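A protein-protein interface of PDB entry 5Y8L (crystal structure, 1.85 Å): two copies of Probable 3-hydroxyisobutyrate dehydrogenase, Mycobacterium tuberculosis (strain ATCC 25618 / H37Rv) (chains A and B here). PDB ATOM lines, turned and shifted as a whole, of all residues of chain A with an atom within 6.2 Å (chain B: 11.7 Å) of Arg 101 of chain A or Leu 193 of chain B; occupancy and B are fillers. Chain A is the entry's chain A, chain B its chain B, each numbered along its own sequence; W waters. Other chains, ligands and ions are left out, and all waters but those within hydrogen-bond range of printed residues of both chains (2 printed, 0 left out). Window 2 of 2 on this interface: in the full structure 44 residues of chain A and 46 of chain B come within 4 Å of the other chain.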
ATOM      1  N   SER A  96     -19.745   6.078  14.247  1.00  0.00           N
ATOM      2  CA  SER A  96     -18.344   6.160  13.927  1.00  0.00           C
ATOM      3  C   SER A  96     -17.434   5.737  15.089  1.00  0.00           C
ATOM      4  O   SER A  96     -17.763   5.868  16.208  1.00  0.00           O
ATOM      5  CB  SER A  96     -17.949   7.575  13.455  1.00  0.00           C
ATOM      6  OG  SER A  96     -17.949   8.466  14.499  1.00  0.00           O
ATOM      7  N   VAL A  97     -16.264   5.269  14.742  1.00  0.00           N
ATOM      8  CA  VAL A  97     -15.279   4.861  15.711  1.00  0.00           C
ATOM      9  C   VAL A  97     -14.960   6.077  16.583  1.00  0.00           C
ATOM     10  O   VAL A  97     -14.871   5.968  17.749  1.00  0.00           O
ATOM     11  CB  VAL A  97     -14.034   4.274  15.037  1.00  0.00           C
ATOM     12  CG1 VAL A  97     -12.931   4.013  16.010  1.00  0.00           C
ATOM     13  CG2 VAL A  97     -14.383   3.055  14.240  1.00  0.00           C
ATOM     14  N   THR A  98     -14.778   7.223  15.951  1.00  0.00           N
ATOM     15  CA  THR A  98     -14.545   8.446  16.751  1.00  0.00           C
ATOM     16  C   THR A  98     -15.625   8.734  17.767  1.00  0.00           C
ATOM     17  O   THR A  98     -15.329   8.984  18.953  1.00  0.00           O
ATOM     18  CB  THR A  98     -14.386   9.681  15.815  1.00  0.00           C
ATOM     19  OG1 THR A  98     -13.312   9.425  14.906  1.00  0.00           O
ATOM     20  CG2 THR A  98     -14.010  10.923  16.602  1.00  0.00           C
ATOM     21  N   ASP A  99     -16.890   8.727  17.317  1.00  0.00           N
ATOM     22  CA  ASP A  99     -18.000   8.965  18.260  1.00  0.00           C
ATOM     23  C   ASP A  99     -18.089   7.871  19.313  1.00  0.00           C
ATOM     24  O   ASP A  99     -18.273   8.174  20.453  1.00  0.00           O
ATOM     25  CB  ASP A  99     -19.334   9.027  17.549  1.00  0.00           C
ATOM     26  CG  ASP A  99     -19.478  10.309  16.702  1.00  0.00           C
ATOM     27  OD1 ASP A  99     -18.647  11.221  16.808  1.00  0.00           O
ATOM     28  OD2 ASP A  99     -20.399  10.400  15.881  1.00  0.00           O
ATOM     29  N   ALA A 100     -17.881   6.615  18.924  1.00  0.00           N
ATOM     30  CA  ALA A 100     -17.846   5.560  19.909  1.00  0.00           C
ATOM     31  C   ALA A 100     -16.861   5.800  21.017  1.00  0.00           C
ATOM     32  O   ALA A 100     -17.169   5.625  22.200  1.00  0.00           O
ATOM     33  CB  ALA A 100     -17.543   4.201  19.249  1.00  0.00           C
ATOM     34  N   ARG A 101     -15.643   6.116  20.637  1.00  0.00           N
ATOM     35  CA  ARG A 101     -14.565   6.392  21.650  1.00  0.00           C
ATOM     36  C   ARG A 101     -14.808   7.604  22.522  1.00  0.00           C
ATOM     37  O   ARG A 101     -14.531   7.588  23.734  1.00  0.00           O
ATOM     38  CB  ARG A 101     -13.205   6.480  20.989  1.00  0.00           C
ATOM     39  CG  ARG A 101     -12.797   5.099  20.500  1.00  0.00           C
ATOM     40  CD  ARG A 101     -11.548   5.137  19.655  1.00  0.00           C
ATOM     41  NE  ARG A 101     -11.157   3.766  19.322  1.00  0.00           N
ATOM     42  CZ  ARG A 101     -10.298   3.438  18.365  1.00  0.00           C
ATOM     43  NH1 ARG A 101      -9.810   4.375  17.537  1.00  0.00           N
ATOM     44  NH2 ARG A 101     -10.014   2.142  18.198  1.00  0.00           N
ATOM     45  N   GLU A 102     -15.469   8.585  21.962  1.00  0.00           N
ATOM     46  CA  GLU A 102     -15.815   9.755  22.722  1.00  0.00           C
ATOM     47  C   GLU A 102     -16.883   9.456  23.733  1.00  0.00           C
ATOM     48  O   GLU A 102     -16.752   9.918  24.895  1.00  0.00           O
ATOM     49  CB  GLU A 102     -16.292  10.864  21.811  1.00  0.00           C
ATOM     50  CG  GLU A 102     -16.746  12.107  22.560  1.00  0.00           C
ATOM     51  CD  GLU A 102     -17.325  13.164  21.614  1.00  0.00           C
ATOM     52  OE1 GLU A 102     -16.797  13.304  20.487  1.00  0.00           O
ATOM     53  OE2 GLU A 102     -18.314  13.831  22.000  1.00  0.00           O
ATOM     54  N   VAL A 103     -17.950   8.736  23.350  1.00  0.00           N
ATOM     55  CA  VAL A 103     -19.008   8.437  24.299  1.00  0.00           C
ATOM     56  C   VAL A 103     -18.565   7.416  25.345  1.00  0.00           C
ATOM     57  O   VAL A 103     -19.029   7.480  26.479  1.00  0.00           O
ATOM     58  CB  VAL A 103     -20.375   8.080  23.646  1.00  0.00           C
ATOM     59  CG1 VAL A 103     -20.803   9.184  22.642  1.00  0.00           C
ATOM     60  CG2 VAL A 103     -20.383   6.698  22.974  1.00  0.00           C
ATOM     61  N   HIS A 104     -17.627   6.517  24.988  1.00  0.00           N
ATOM     62  CA  HIS A 104     -17.023   5.617  25.957  1.00  0.00           C
ATOM     63  C   HIS A 104     -16.294   6.424  27.061  1.00  0.00           C
ATOM     64  O   HIS A 104     -16.459   6.171  28.258  1.00  0.00           O
ATOM     65  CB  HIS A 104     -16.043   4.691  25.236  1.00  0.00           C
ATOM     66  CG  HIS A 104     -15.263   3.846  26.135  1.00  0.00           C
ATOM     67  ND1 HIS A 104     -15.784   2.719  26.713  1.00  0.00           N
ATOM     68  CD2 HIS A 104     -14.005   3.976  26.603  1.00  0.00           C
ATOM     69  CE1 HIS A 104     -14.869   2.184  27.500  1.00  0.00           C
ATOM     70  NE2 HIS A 104     -13.776   2.920  27.435  1.00  0.00           N
ATOM     71  N   ALA A 105     -15.439   7.351  26.654  1.00  0.00           N
ATOM     72  CA  ALA A 105     -14.653   8.109  27.607  1.00  0.00           C
ATOM     73  C   ALA A 105     -15.584   8.980  28.449  1.00  0.00           C
ATOM     74  O   ALA A 105     -15.361   9.129  29.636  1.00  0.00           O
ATOM     75  CB  ALA A 105     -13.616   8.983  26.891  1.00  0.00           C
ATOM     76  N   LEU A 106     -16.634   9.529  27.853  1.00  0.00           N
ATOM     77  CA  LEU A 106     -17.623  10.261  28.636  1.00  0.00           C
ATOM     78  C   LEU A 106     -18.268   9.415  29.737  1.00  0.00           C
ATOM     79  O   LEU A 106     -18.329   9.795  30.886  1.00  0.00           O
ATOM     80  CB  LEU A 106     -18.633  10.876  27.664  1.00  0.00           C
ATOM     81  CG  LEU A 106     -19.719  11.708  28.260  1.00  0.00           C
ATOM     82  CD1 LEU A 106     -19.164  12.952  28.954  1.00  0.00           C
ATOM     83  CD2 LEU A 106     -20.694  12.041  27.087  1.00  0.00           C
ATOM     84  N   ALA A 161     -10.239  -2.938  22.262  1.00  0.00           N
ATOM     85  CA  ALA A 161     -10.534  -1.830  23.210  1.00  0.00           C
ATOM     86  C   ALA A 161     -11.715  -0.965  22.605  1.00  0.00           C
ATOM     87  O   ALA A 161     -12.113  -1.194  21.437  1.00  0.00           O
ATOM     88  CB  ALA A 161      -9.288  -1.029  23.500  1.00  0.00           C
ATOM     89  N   ALA A 162     -12.193   0.006  23.369  1.00  0.00           N
ATOM     90  CA  ALA A 162     -13.358   0.816  23.012  1.00  0.00           C
ATOM     91  C   ALA A 162     -13.172   1.337  21.595  1.00  0.00           C
ATOM     92  O   ALA A 162     -12.104   1.802  21.200  1.00  0.00           O
ATOM     93  CB  ALA A 162     -13.528   1.970  23.960  1.00  0.00           C
ATOM     94  N   GLY A 163     -14.209   1.173  20.835  1.00  0.00           N
ATOM     95  CA  GLY A 163     -14.277   1.536  19.425  1.00  0.00           C
ATOM     96  C   GLY A 163     -13.980   0.382  18.449  1.00  0.00           C
ATOM     97  O   GLY A 163     -14.329   0.451  17.264  1.00  0.00           O
ATOM     98  N   ALA A 164     -13.406  -0.722  18.925  1.00  0.00           N
ATOM     99  CA  ALA A 164     -13.027  -1.843  18.054  1.00  0.00           C
ATOM    100  C   ALA A 164     -14.234  -2.589  17.454  1.00  0.00           C
ATOM    101  O   ALA A 164     -14.131  -3.235  16.373  1.00  0.00           O
ATOM    102  CB  ALA A 164     -12.124  -2.835  18.820  1.00  0.00           C
ATOM    103  N   ALA A 167     -15.260  -0.501  14.588  1.00  0.00           N
ATOM    104  CA  ALA A 167     -14.258  -0.580  13.535  1.00  0.00           C
ATOM    105  C   ALA A 167     -14.364  -1.901  12.788  1.00  0.00           C
ATOM    106  O   ALA A 167     -14.240  -1.947  11.538  1.00  0.00           O
ATOM    107  CB  ALA A 167     -12.850  -0.480  14.122  1.00  0.00           C
ATOM    108  N   VAL A 170     -17.510  -1.842  10.563  1.00  0.00           N
ATOM    109  CA  VAL A 170     -17.351  -0.942   9.394  1.00  0.00           C
ATOM    110  C   VAL A 170     -16.388  -1.540   8.327  1.00  0.00           C
ATOM    111  O   VAL A 170     -16.656  -1.460   7.085  1.00  0.00           O
ATOM    112  CB  VAL A 170     -17.073   0.519   9.848  1.00  0.00           C
ATOM    113  CG1 VAL A 170     -15.617   0.797  10.131  1.00  0.00           C
ATOM    114  CG2 VAL A 170     -17.586   1.495   8.808  1.00  0.00           C
ATOM    115  N   CYS A 171     -15.328  -2.192   8.795  1.00  0.00           N
ATOM    116  CA  CYS A 171     -14.372  -2.822   7.897  1.00  0.00           C
ATOM    117  C   CYS A 171     -14.988  -4.007   7.161  1.00  0.00           C
ATOM    118  O   CYS A 171     -14.886  -4.110   5.910  1.00  0.00           O
ATOM    119  CB  CYS A 171     -13.068  -3.230   8.652  1.00  0.00           C
ATOM    120  SG  CYS A 171     -12.036  -1.802   9.107  1.00  0.00           S
ATOM    121  N   ALA A 252     -14.388   7.039   8.673  1.00  0.00           N
ATOM    122  CA  ALA A 252     -13.204   6.483   9.203  1.00  0.00           C
ATOM    123  C   ALA A 252     -12.004   6.716   8.259  1.00  0.00           C
ATOM    124  O   ALA A 252     -10.894   7.026   8.734  1.00  0.00           O
ATOM    125  CB  ALA A 252     -13.385   5.045   9.471  1.00  0.00           C
ATOM    126  N   VAL A 253     -12.210   6.550   6.962  1.00  0.00           N
ATOM    127  CA  VAL A 253     -11.148   6.768   5.963  1.00  0.00           C
ATOM    128  C   VAL A 253     -10.657   8.237   6.015  1.00  0.00           C
ATOM    129  O   VAL A 253      -9.451   8.500   6.061  1.00  0.00           O
ATOM    130  CB  VAL A 253     -11.632   6.369   4.558  1.00  0.00           C
ATOM    131  CG1 VAL A 253     -10.679   6.918   3.472  1.00  0.00           C
ATOM    132  CG2 VAL A 253     -11.705   4.856   4.498  1.00  0.00           C
ATOM    133  N   ALA A 255     -11.058  10.411   8.620  1.00  0.00           N
ATOM    134  CA  ALA A 255     -10.429  10.667   9.895  1.00  0.00           C
ATOM    135  C   ALA A 255      -8.995  10.134   9.960  1.00  0.00           C
ATOM    136  O   ALA A 255      -8.162  10.689  10.647  1.00  0.00           O
ATOM    137  CB  ALA A 255     -11.247  10.054  11.000  1.00  0.00           C
ATOM    138  N   THR A 256      -8.715   8.978   9.362  1.00  0.00           N
ATOM    139  CA  THR A 256      -7.376   8.356   9.481  1.00  0.00           C
ATOM    140  C   THR A 256      -6.397   8.730   8.368  1.00  0.00           C
ATOM    141  O   THR A 256      -5.200   8.401   8.452  1.00  0.00           O
ATOM    142  CB  THR A 256      -7.492   6.829   9.473  1.00  0.00           C
ATOM    143  OG1 THR A 256      -8.132   6.422   8.272  1.00  0.00           O
ATOM    144  CG2 THR A 256      -8.352   6.342  10.687  1.00  0.00           C
ATOM    145  N   ALA B 184      -7.180  -5.892   1.463  1.00  0.00           N
ATOM    146  CA  ALA B 184      -6.026  -5.111   1.798  1.00  0.00           C
ATOM    147  C   ALA B 184      -6.440  -3.724   2.399  1.00  0.00           C
ATOM    148  O   ALA B 184      -5.845  -3.290   3.420  1.00  0.00           O
ATOM    149  CB  ALA B 184      -5.079  -4.925   0.618  1.00  0.00           C
ATOM    150  N   GLU B 185      -7.432  -3.075   1.774  1.00  0.00           N
ATOM    151  CA  GLU B 185      -7.918  -1.807   2.225  1.00  0.00           C
ATOM    152  C   GLU B 185      -8.473  -1.892   3.655  1.00  0.00           C
ATOM    153  O   GLU B 185      -8.182  -1.030   4.474  1.00  0.00           O
ATOM    154  CB  GLU B 185      -9.017  -1.280   1.349  1.00  0.00           C
ATOM    155  CG  GLU B 185      -8.567  -0.978  -0.091  1.00  0.00           C
ATOM    156  CD  GLU B 185      -9.731  -0.472  -0.950  1.00  0.00           C
ATOM    157  OE1 GLU B 185     -10.897  -0.312  -0.452  1.00  0.00           O
ATOM    158  OE2 GLU B 185      -9.450  -0.199  -2.151  1.00  0.00           O
ATOM    159  N   ALA B 186      -9.183  -2.972   3.944  1.00  0.00           N
ATOM    160  CA  ALA B 186      -9.730  -3.210   5.272  1.00  0.00           C
ATOM    161  C   ALA B 186      -8.634  -3.389   6.324  1.00  0.00           C
ATOM    162  O   ALA B 186      -8.741  -2.787   7.362  1.00  0.00           O
ATOM    163  CB  ALA B 186     -10.658  -4.414   5.265  1.00  0.00           C
ATOM    164  N   PHE B 187      -7.619  -4.232   6.069  1.00  0.00           N
ATOM    165  CA  PHE B 187      -6.524  -4.370   7.010  1.00  0.00           C
ATOM    166  C   PHE B 187      -5.741  -3.076   7.285  1.00  0.00           C
ATOM    167  O   PHE B 187      -5.352  -2.835   8.423  1.00  0.00           O
ATOM    168  CB  PHE B 187      -5.566  -5.500   6.624  1.00  0.00           C
ATOM    169  CG  PHE B 187      -6.080  -6.834   6.973  1.00  0.00           C
ATOM    170  CD1 PHE B 187      -5.947  -7.296   8.275  1.00  0.00           C
ATOM    171  CD2 PHE B 187      -6.731  -7.635   6.043  1.00  0.00           C
ATOM    172  CE1 PHE B 187      -6.419  -8.544   8.643  1.00  0.00           C
ATOM    173  CE2 PHE B 187      -7.207  -8.914   6.410  1.00  0.00           C
ATOM    174  CZ  PHE B 187      -7.079  -9.351   7.732  1.00  0.00           C
ATOM    175  N   VAL B 188      -5.569  -2.224   6.283  1.00  0.00           N
ATOM    176  CA  VAL B 188      -4.820  -1.009   6.504  1.00  0.00           C
ATOM    177  C   VAL B 188      -5.679  -0.001   7.270  1.00  0.00           C
ATOM    178  O   VAL B 188      -5.182   0.616   8.171  1.00  0.00           O
ATOM    179  CB  VAL B 188      -4.271  -0.421   5.206  1.00  0.00           C
ATOM    180  CG1 VAL B 188      -3.478   0.853   5.515  1.00  0.00           C
ATOM    181  CG2 VAL B 188      -3.286  -1.406   4.606  1.00  0.00           C
ATOM    182  N   LEU B 189      -6.964   0.086   6.941  1.00  0.00           N
ATOM    183  CA  LEU B 189      -7.922   0.946   7.687  1.00  0.00           C
ATOM    184  C   LEU B 189      -7.979   0.495   9.148  1.00  0.00           C
ATOM    185  O   LEU B 189      -7.913   1.292  10.055  1.00  0.00           O
ATOM    186  CB  LEU B 189      -9.293   0.922   7.038  1.00  0.00           C
ATOM    187  CG  LEU B 189     -10.362   1.764   7.735  1.00  0.00           C
ATOM    188  CD1 LEU B 189     -10.002   3.256   7.868  1.00  0.00           C
ATOM    189  CD2 LEU B 189     -11.669   1.643   7.008  1.00  0.00           C
ATOM    190  N   ALA B 190      -8.043  -0.801   9.381  1.00  0.00           N
ATOM    191  CA  ALA B 190      -8.082  -1.370  10.741  1.00  0.00           C
ATOM    192  C   ALA B 190      -6.859  -0.946  11.507  1.00  0.00           C
ATOM    193  O   ALA B 190      -6.947  -0.469  12.608  1.00  0.00           O
ATOM    194  CB  ALA B 190      -8.152  -2.899  10.708  1.00  0.00           C
ATOM    195  N   GLU B 191      -5.713  -1.090  10.915  1.00  0.00           N
ATOM    196  CA  GLU B 191      -4.448  -0.654  11.537  1.00  0.00           C
ATOM    197  C   GLU B 191      -4.503   0.821  11.952  1.00  0.00           C
ATOM    198  O   GLU B 191      -4.126   1.165  13.024  1.00  0.00           O
ATOM    199  CB  GLU B 191      -3.334  -0.915  10.502  1.00  0.00           C
ATOM    200  CG  GLU B 191      -1.920  -0.430  10.739  1.00  0.00           C
ATOM    201  CD  GLU B 191      -1.145  -0.378   9.362  1.00  0.00           C
ATOM    202  OE1 GLU B 191      -1.137  -1.394   8.580  1.00  0.00           O
ATOM    203  OE2 GLU B 191      -0.597   0.716   9.020  1.00  0.00           O
ATOM    204  N   LYS B 192      -4.973   1.688  11.073  1.00  0.00           N
ATOM    205  CA  LYS B 192      -5.054   3.095  11.368  1.00  0.00           C
ATOM    206  C   LYS B 192      -6.089   3.426  12.439  1.00  0.00           C
ATOM    207  O   LYS B 192      -5.973   4.434  13.107  1.00  0.00           O
ATOM    208  CB  LYS B 192      -5.347   3.896  10.112  1.00  0.00           C
ATOM    209  CG  LYS B 192      -4.143   3.852   9.101  1.00  0.00           C
ATOM    210  CD  LYS B 192      -4.422   4.763   7.906  1.00  0.00           C
ATOM    211  CE  LYS B 192      -3.142   5.362   7.293  1.00  0.00           C
ATOM    212  NZ  LYS B 192      -2.616   4.428   6.291  1.00  0.00           N
ATOM    213  N   LEU B 193      -7.153   2.628  12.531  1.00  0.00           N
ATOM    214  CA  LEU B 193      -8.174   2.785  13.557  1.00  0.00           C
ATOM    215  C   LEU B 193      -7.732   2.145  14.870  1.00  0.00           C
ATOM    216  O   LEU B 193      -8.468   2.193  15.789  1.00  0.00           O
ATOM    217  CB  LEU B 193      -9.508   2.149  13.109  1.00  0.00           C
ATOM    218  CG  LEU B 193     -10.238   2.857  11.995  1.00  0.00           C
ATOM    219  CD1 LEU B 193     -11.384   1.991  11.507  1.00  0.00           C
ATOM    220  CD2 LEU B 193     -10.751   4.238  12.334  1.00  0.00           C
ATOM    221  N   GLY B 194      -6.569   1.524  14.951  1.00  0.00           N
ATOM    222  CA  GLY B 194      -6.176   0.756  16.127  1.00  0.00           C
ATOM    223  C   GLY B 194      -6.873  -0.578  16.354  1.00  0.00           C
ATOM    224  O   GLY B 194      -6.759  -1.139  17.441  1.00  0.00           O
ATOM    225  N   LEU B 195      -7.477  -1.166  15.316  1.00  0.00           N
ATOM    226  CA  LEU B 195      -8.056  -2.519  15.427  1.00  0.00           C
ATOM    227  C   LEU B 195      -6.971  -3.533  14.975  1.00  0.00           C
ATOM    228  O   LEU B 195      -6.384  -3.379  13.911  1.00  0.00           O
ATOM    229  CB  LEU B 195      -9.326  -2.604  14.572  1.00  0.00           C
ATOM    230  CG  LEU B 195      -9.944  -3.966  14.329  1.00  0.00           C
ATOM    231  CD1 LEU B 195     -10.533  -4.577  15.606  1.00  0.00           C
ATOM    232  CD2 LEU B 195     -10.969  -3.818  13.254  1.00  0.00           C
ATOM    233  N   SER B 196      -6.674  -4.531  15.795  1.00  0.00           N
ATOM    234  CA  SER B 196      -5.589  -5.442  15.488  1.00  0.00           C
ATOM    235  C   SER B 196      -5.915  -6.312  14.262  1.00  0.00           C
ATOM    236  O   SER B 196      -7.075  -6.575  13.946  1.00  0.00           O
ATOM    237  CB  SER B 196      -5.191  -6.327  16.677  1.00  0.00           C
ATOM    238  OG  SER B 196      -6.019  -7.432  16.795  1.00  0.00           O
ATOM    239  N   ALA B 197      -4.859  -6.740  13.577  1.00  0.00           N
ATOM    240  CA  ALA B 197      -4.995  -7.529  12.392  1.00  0.00           C
ATOM    241  C   ALA B 197      -5.600  -8.857  12.762  1.00  0.00           C
ATOM    242  O   ALA B 197      -6.459  -9.358  12.020  1.00  0.00           O
ATOM    243  CB  ALA B 197      -3.646  -7.748  11.743  1.00  0.00           C
ATOM    244  N   SER B 199      -7.664  -9.431  15.174  1.00  0.00           N
ATOM    245  CA  SER B 199      -9.053  -9.152  15.491  1.00  0.00           C
ATOM    246  C   SER B 199      -9.887  -8.975  14.216  1.00  0.00           C
ATOM    247  O   SER B 199     -10.971  -9.561  14.077  1.00  0.00           O
ATOM    248  CB  SER B 199      -9.169  -7.915  16.404  1.00  0.00           C
ATOM    249  OG  SER B 199      -8.767  -8.213  17.735  1.00  0.00           O
ATOM    250  N   LEU B 200      -9.374  -8.219  13.261  1.00  0.00           N
ATOM    251  CA  LEU B 200     -10.123  -7.987  11.995  1.00  0.00           C
ATOM    252  C   LEU B 200     -10.253  -9.323  11.256  1.00  0.00           C
ATOM    253  O   LEU B 200     -11.321  -9.660  10.733  1.00  0.00           O
ATOM    254  CB  LEU B 200      -9.456  -6.957  11.112  1.00  0.00           C
ATOM    255  CG  LEU B 200     -10.198  -6.809   9.776  1.00  0.00           C
ATOM    256  CD1 LEU B 200     -11.545  -6.212   9.976  1.00  0.00           C
ATOM    257  CD2 LEU B 200      -9.414  -5.947   8.774  1.00  0.00           C
ATOM    258  N   ILE B 204     -13.924 -10.828  10.108  1.00  0.00           N
ATOM    259  CA  ILE B 204     -14.284 -10.945   8.714  1.00  0.00           C
ATOM    260  C   ILE B 204     -14.441 -12.396   8.343  1.00  0.00           C
ATOM    261  O   ILE B 204     -15.390 -12.746   7.614  1.00  0.00           O
ATOM    262  CB  ILE B 204     -13.259 -10.277   7.756  1.00  0.00           C
ATOM    263  CG1 ILE B 204     -13.201  -8.790   8.023  1.00  0.00           C
ATOM    264  CG2 ILE B 204     -13.664 -10.482   6.304  1.00  0.00           C
ATOM    265  CD1 ILE B 204     -12.435  -7.966   6.944  1.00  0.00           C
ATOM    266  N   LEU B 289      -1.142   0.934  -0.265  1.00  0.00           N
ATOM    267  CA  LEU B 289      -2.153   1.594   0.555  1.00  0.00           C
ATOM    268  C   LEU B 289      -1.543   2.130   1.841  1.00  0.00           C
ATOM    269  O   LEU B 289      -2.260   2.676   2.680  1.00  0.00           O
ATOM    270  CB  LEU B 289      -3.208   0.574   0.899  1.00  0.00           C
ATOM    271  CG  LEU B 289      -3.875  -0.144  -0.258  1.00  0.00           C
ATOM    272  CD1 LEU B 289      -4.763  -1.265   0.320  1.00  0.00           C
ATOM    273  CD2 LEU B 289      -4.666   0.791  -1.209  1.00  0.00           C
ATOM    274  N   ARG B 290      -0.241   1.928   2.020  1.00  0.00           N
ATOM    275  CA  ARG B 290       0.519   2.489   3.143  1.00  0.00           C
ATOM    276  C   ARG B 290       1.580   3.506   2.707  1.00  0.00           C
ATOM    277  O   ARG B 290       2.082   3.415   1.573  1.00  0.00           O
ATOM    278  CB  ARG B 290       1.271   1.350   3.810  1.00  0.00           C
ATOM    279  CG  ARG B 290       0.397   0.181   4.272  1.00  0.00           C
ATOM    280  CD  ARG B 290       1.100  -0.506   5.408  1.00  0.00           C
ATOM    281  NE  ARG B 290       0.425  -1.619   6.071  1.00  0.00           N
ATOM    282  CZ  ARG B 290       0.565  -2.899   5.721  1.00  0.00           C
ATOM    283  NH1 ARG B 290       1.323  -3.247   4.667  1.00  0.00           N
ATOM    284  NH2 ARG B 290      -0.063  -3.847   6.423  1.00  0.00           N
HETATM  285  O   HOH W   1      -8.332  -2.367  19.779  1.00  0.00           O
HETATM  286  O   HOH W   2      -7.273   5.269  15.702  1.00  0.00           O
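O of Leu 193 of chain B sits at hydrogen-bond distance from NH2 of Arg 101 of chain A, 2.9 Å away.
Water W2 lies within hydrogen-bond range of O of Lys 192 of chain B, NH1 of Arg 101 of chain A and O of Leu 193 of chain B.
Water W1 lies within hydrogen-bond range of O of Gly 194 of chain B (3.1 Å) and N of Ala 161 of chain A (3.2 Å).
The guanidinium group of Arg 101 of chain A sits at hydrogen-bond distance from the backbone carbonyl oxygen of Ala 162 of chain A, 2.9 Å away.
The side-chain sulfur (SG) of Cys 171 of chain A sits at hydrogen-bond distance from the backbone carbonyl oxygen (O) of Ala 167 of chain A.
O of Ala 252 of chain A is in hydrogen-bond range of OG1 of Thr 256 of chain A, at 2.9 Å.
The side-chain hydroxyl (OG1) of Thr 256 of chain A lies within hydrogen-bond range of the backbone carbonyl oxygen (O) of Val 253 of chain A, at 3.3 Å.
The backbone carbonyl oxygen (O) of Ala 190 of chain B lies within hydrogen-bond range of the backbone NH (N) of Leu 195 of chain B (2.8 Å).
Along chain A the printed residues that touch a printed residue of chain B span positions 101 to 256.
Hydrophobic or aromatic side chains of chain B that line the printed part of chain A: Leu 189, Leu 193, Leu 195 and Leu 200.
Along chain B the printed residues that touch a printed residue of chain A span positions 186 to 200.
Among the printed residues, 11 pairs touch across the chains.
Ala 164 of chain A touches Leu 195 of chain B (O to CD1, 3.9 Å).
CD1 of Leu 193 of chain B touches CB of Ala 167 of chain A, 3.9 Å away.
Ala 167 of chain A touches Leu 195 of chain B.
Cys 171 of chain A touches Ala 186 of chain B.
Cys 171 of chain A touches Leu 200 of chain B.
Ala 252 of chain A touches Leu 189 of chain B (O to CD1, 3.97 Å).
CB of Ala 252 of chain A touches CD2 of Leu 193 of chain B, at 3.97 Å.
Leu 189 of chain B touches Thr 256 of chain A (CD1 to OG1, 3.7 Å).
Thr 256 of chain A touches Lys 192 of chain B.
Leu 193 of chain B touches Thr 256 of chain A.
No residue of chain B comes within 4 Å of Val 97 of chain A.
No residue of chain B comes within 4 Å of Thr 98 of chain A.
Arg 101 of chain A touches just one residue of chain B: Leu 193 (2.9 Å).
No residue of chain B comes within 4 Å of Glu 102 of chain A.
No residue of chain B comes within 4 Å of Ala 105 of chain A.
No residue of chain B comes within 4 Å of Ala 161 of chain A.
No residue of chain B comes within 4 Å of Ala 162 of chain A.
No residue of chain B comes within 4 Å of Gly 163 of chain A.
Of the printed residues of chain B, Ala 164 of chain A touches Leu 195 (3.9 Å).
Of chain B, only Leu 193 (3.9 Å) and Leu 195 (3.9 Å) come within 4 Å of Ala 167 of chain A.
Printed residues of chain B within 4 Å of Cys 171 of chain A: Ala 186 (3.9 Å) and Leu 200 (3.6 Å).
Of chain B, only Leu 189 (3.97 Å) and Leu 193 (3.97 Å) come within 4 Å of Ala 252 of chain A.
No residue of chain B comes within 4 Å of Ala 255 of chain A.
Thr 256 of chain A touches three residues of chain B.
Of the printed residues of chain A, Ala 186 of chain B touches Cys 171.
Glu 191 of chain B touches none of the printed residues of chain A.
Of the printed residues of chain A, Lys 192 of chain B touches Thr 256.
Leu 193 of chain B touches four residues of chain A.
Ile 204 of chain B touches none of the printed residues of chain A.
No position is printed for both chains.
Of the 11 pairs that touch across the chains among the printed residues, none has its exchanged pair printed and touching as well.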
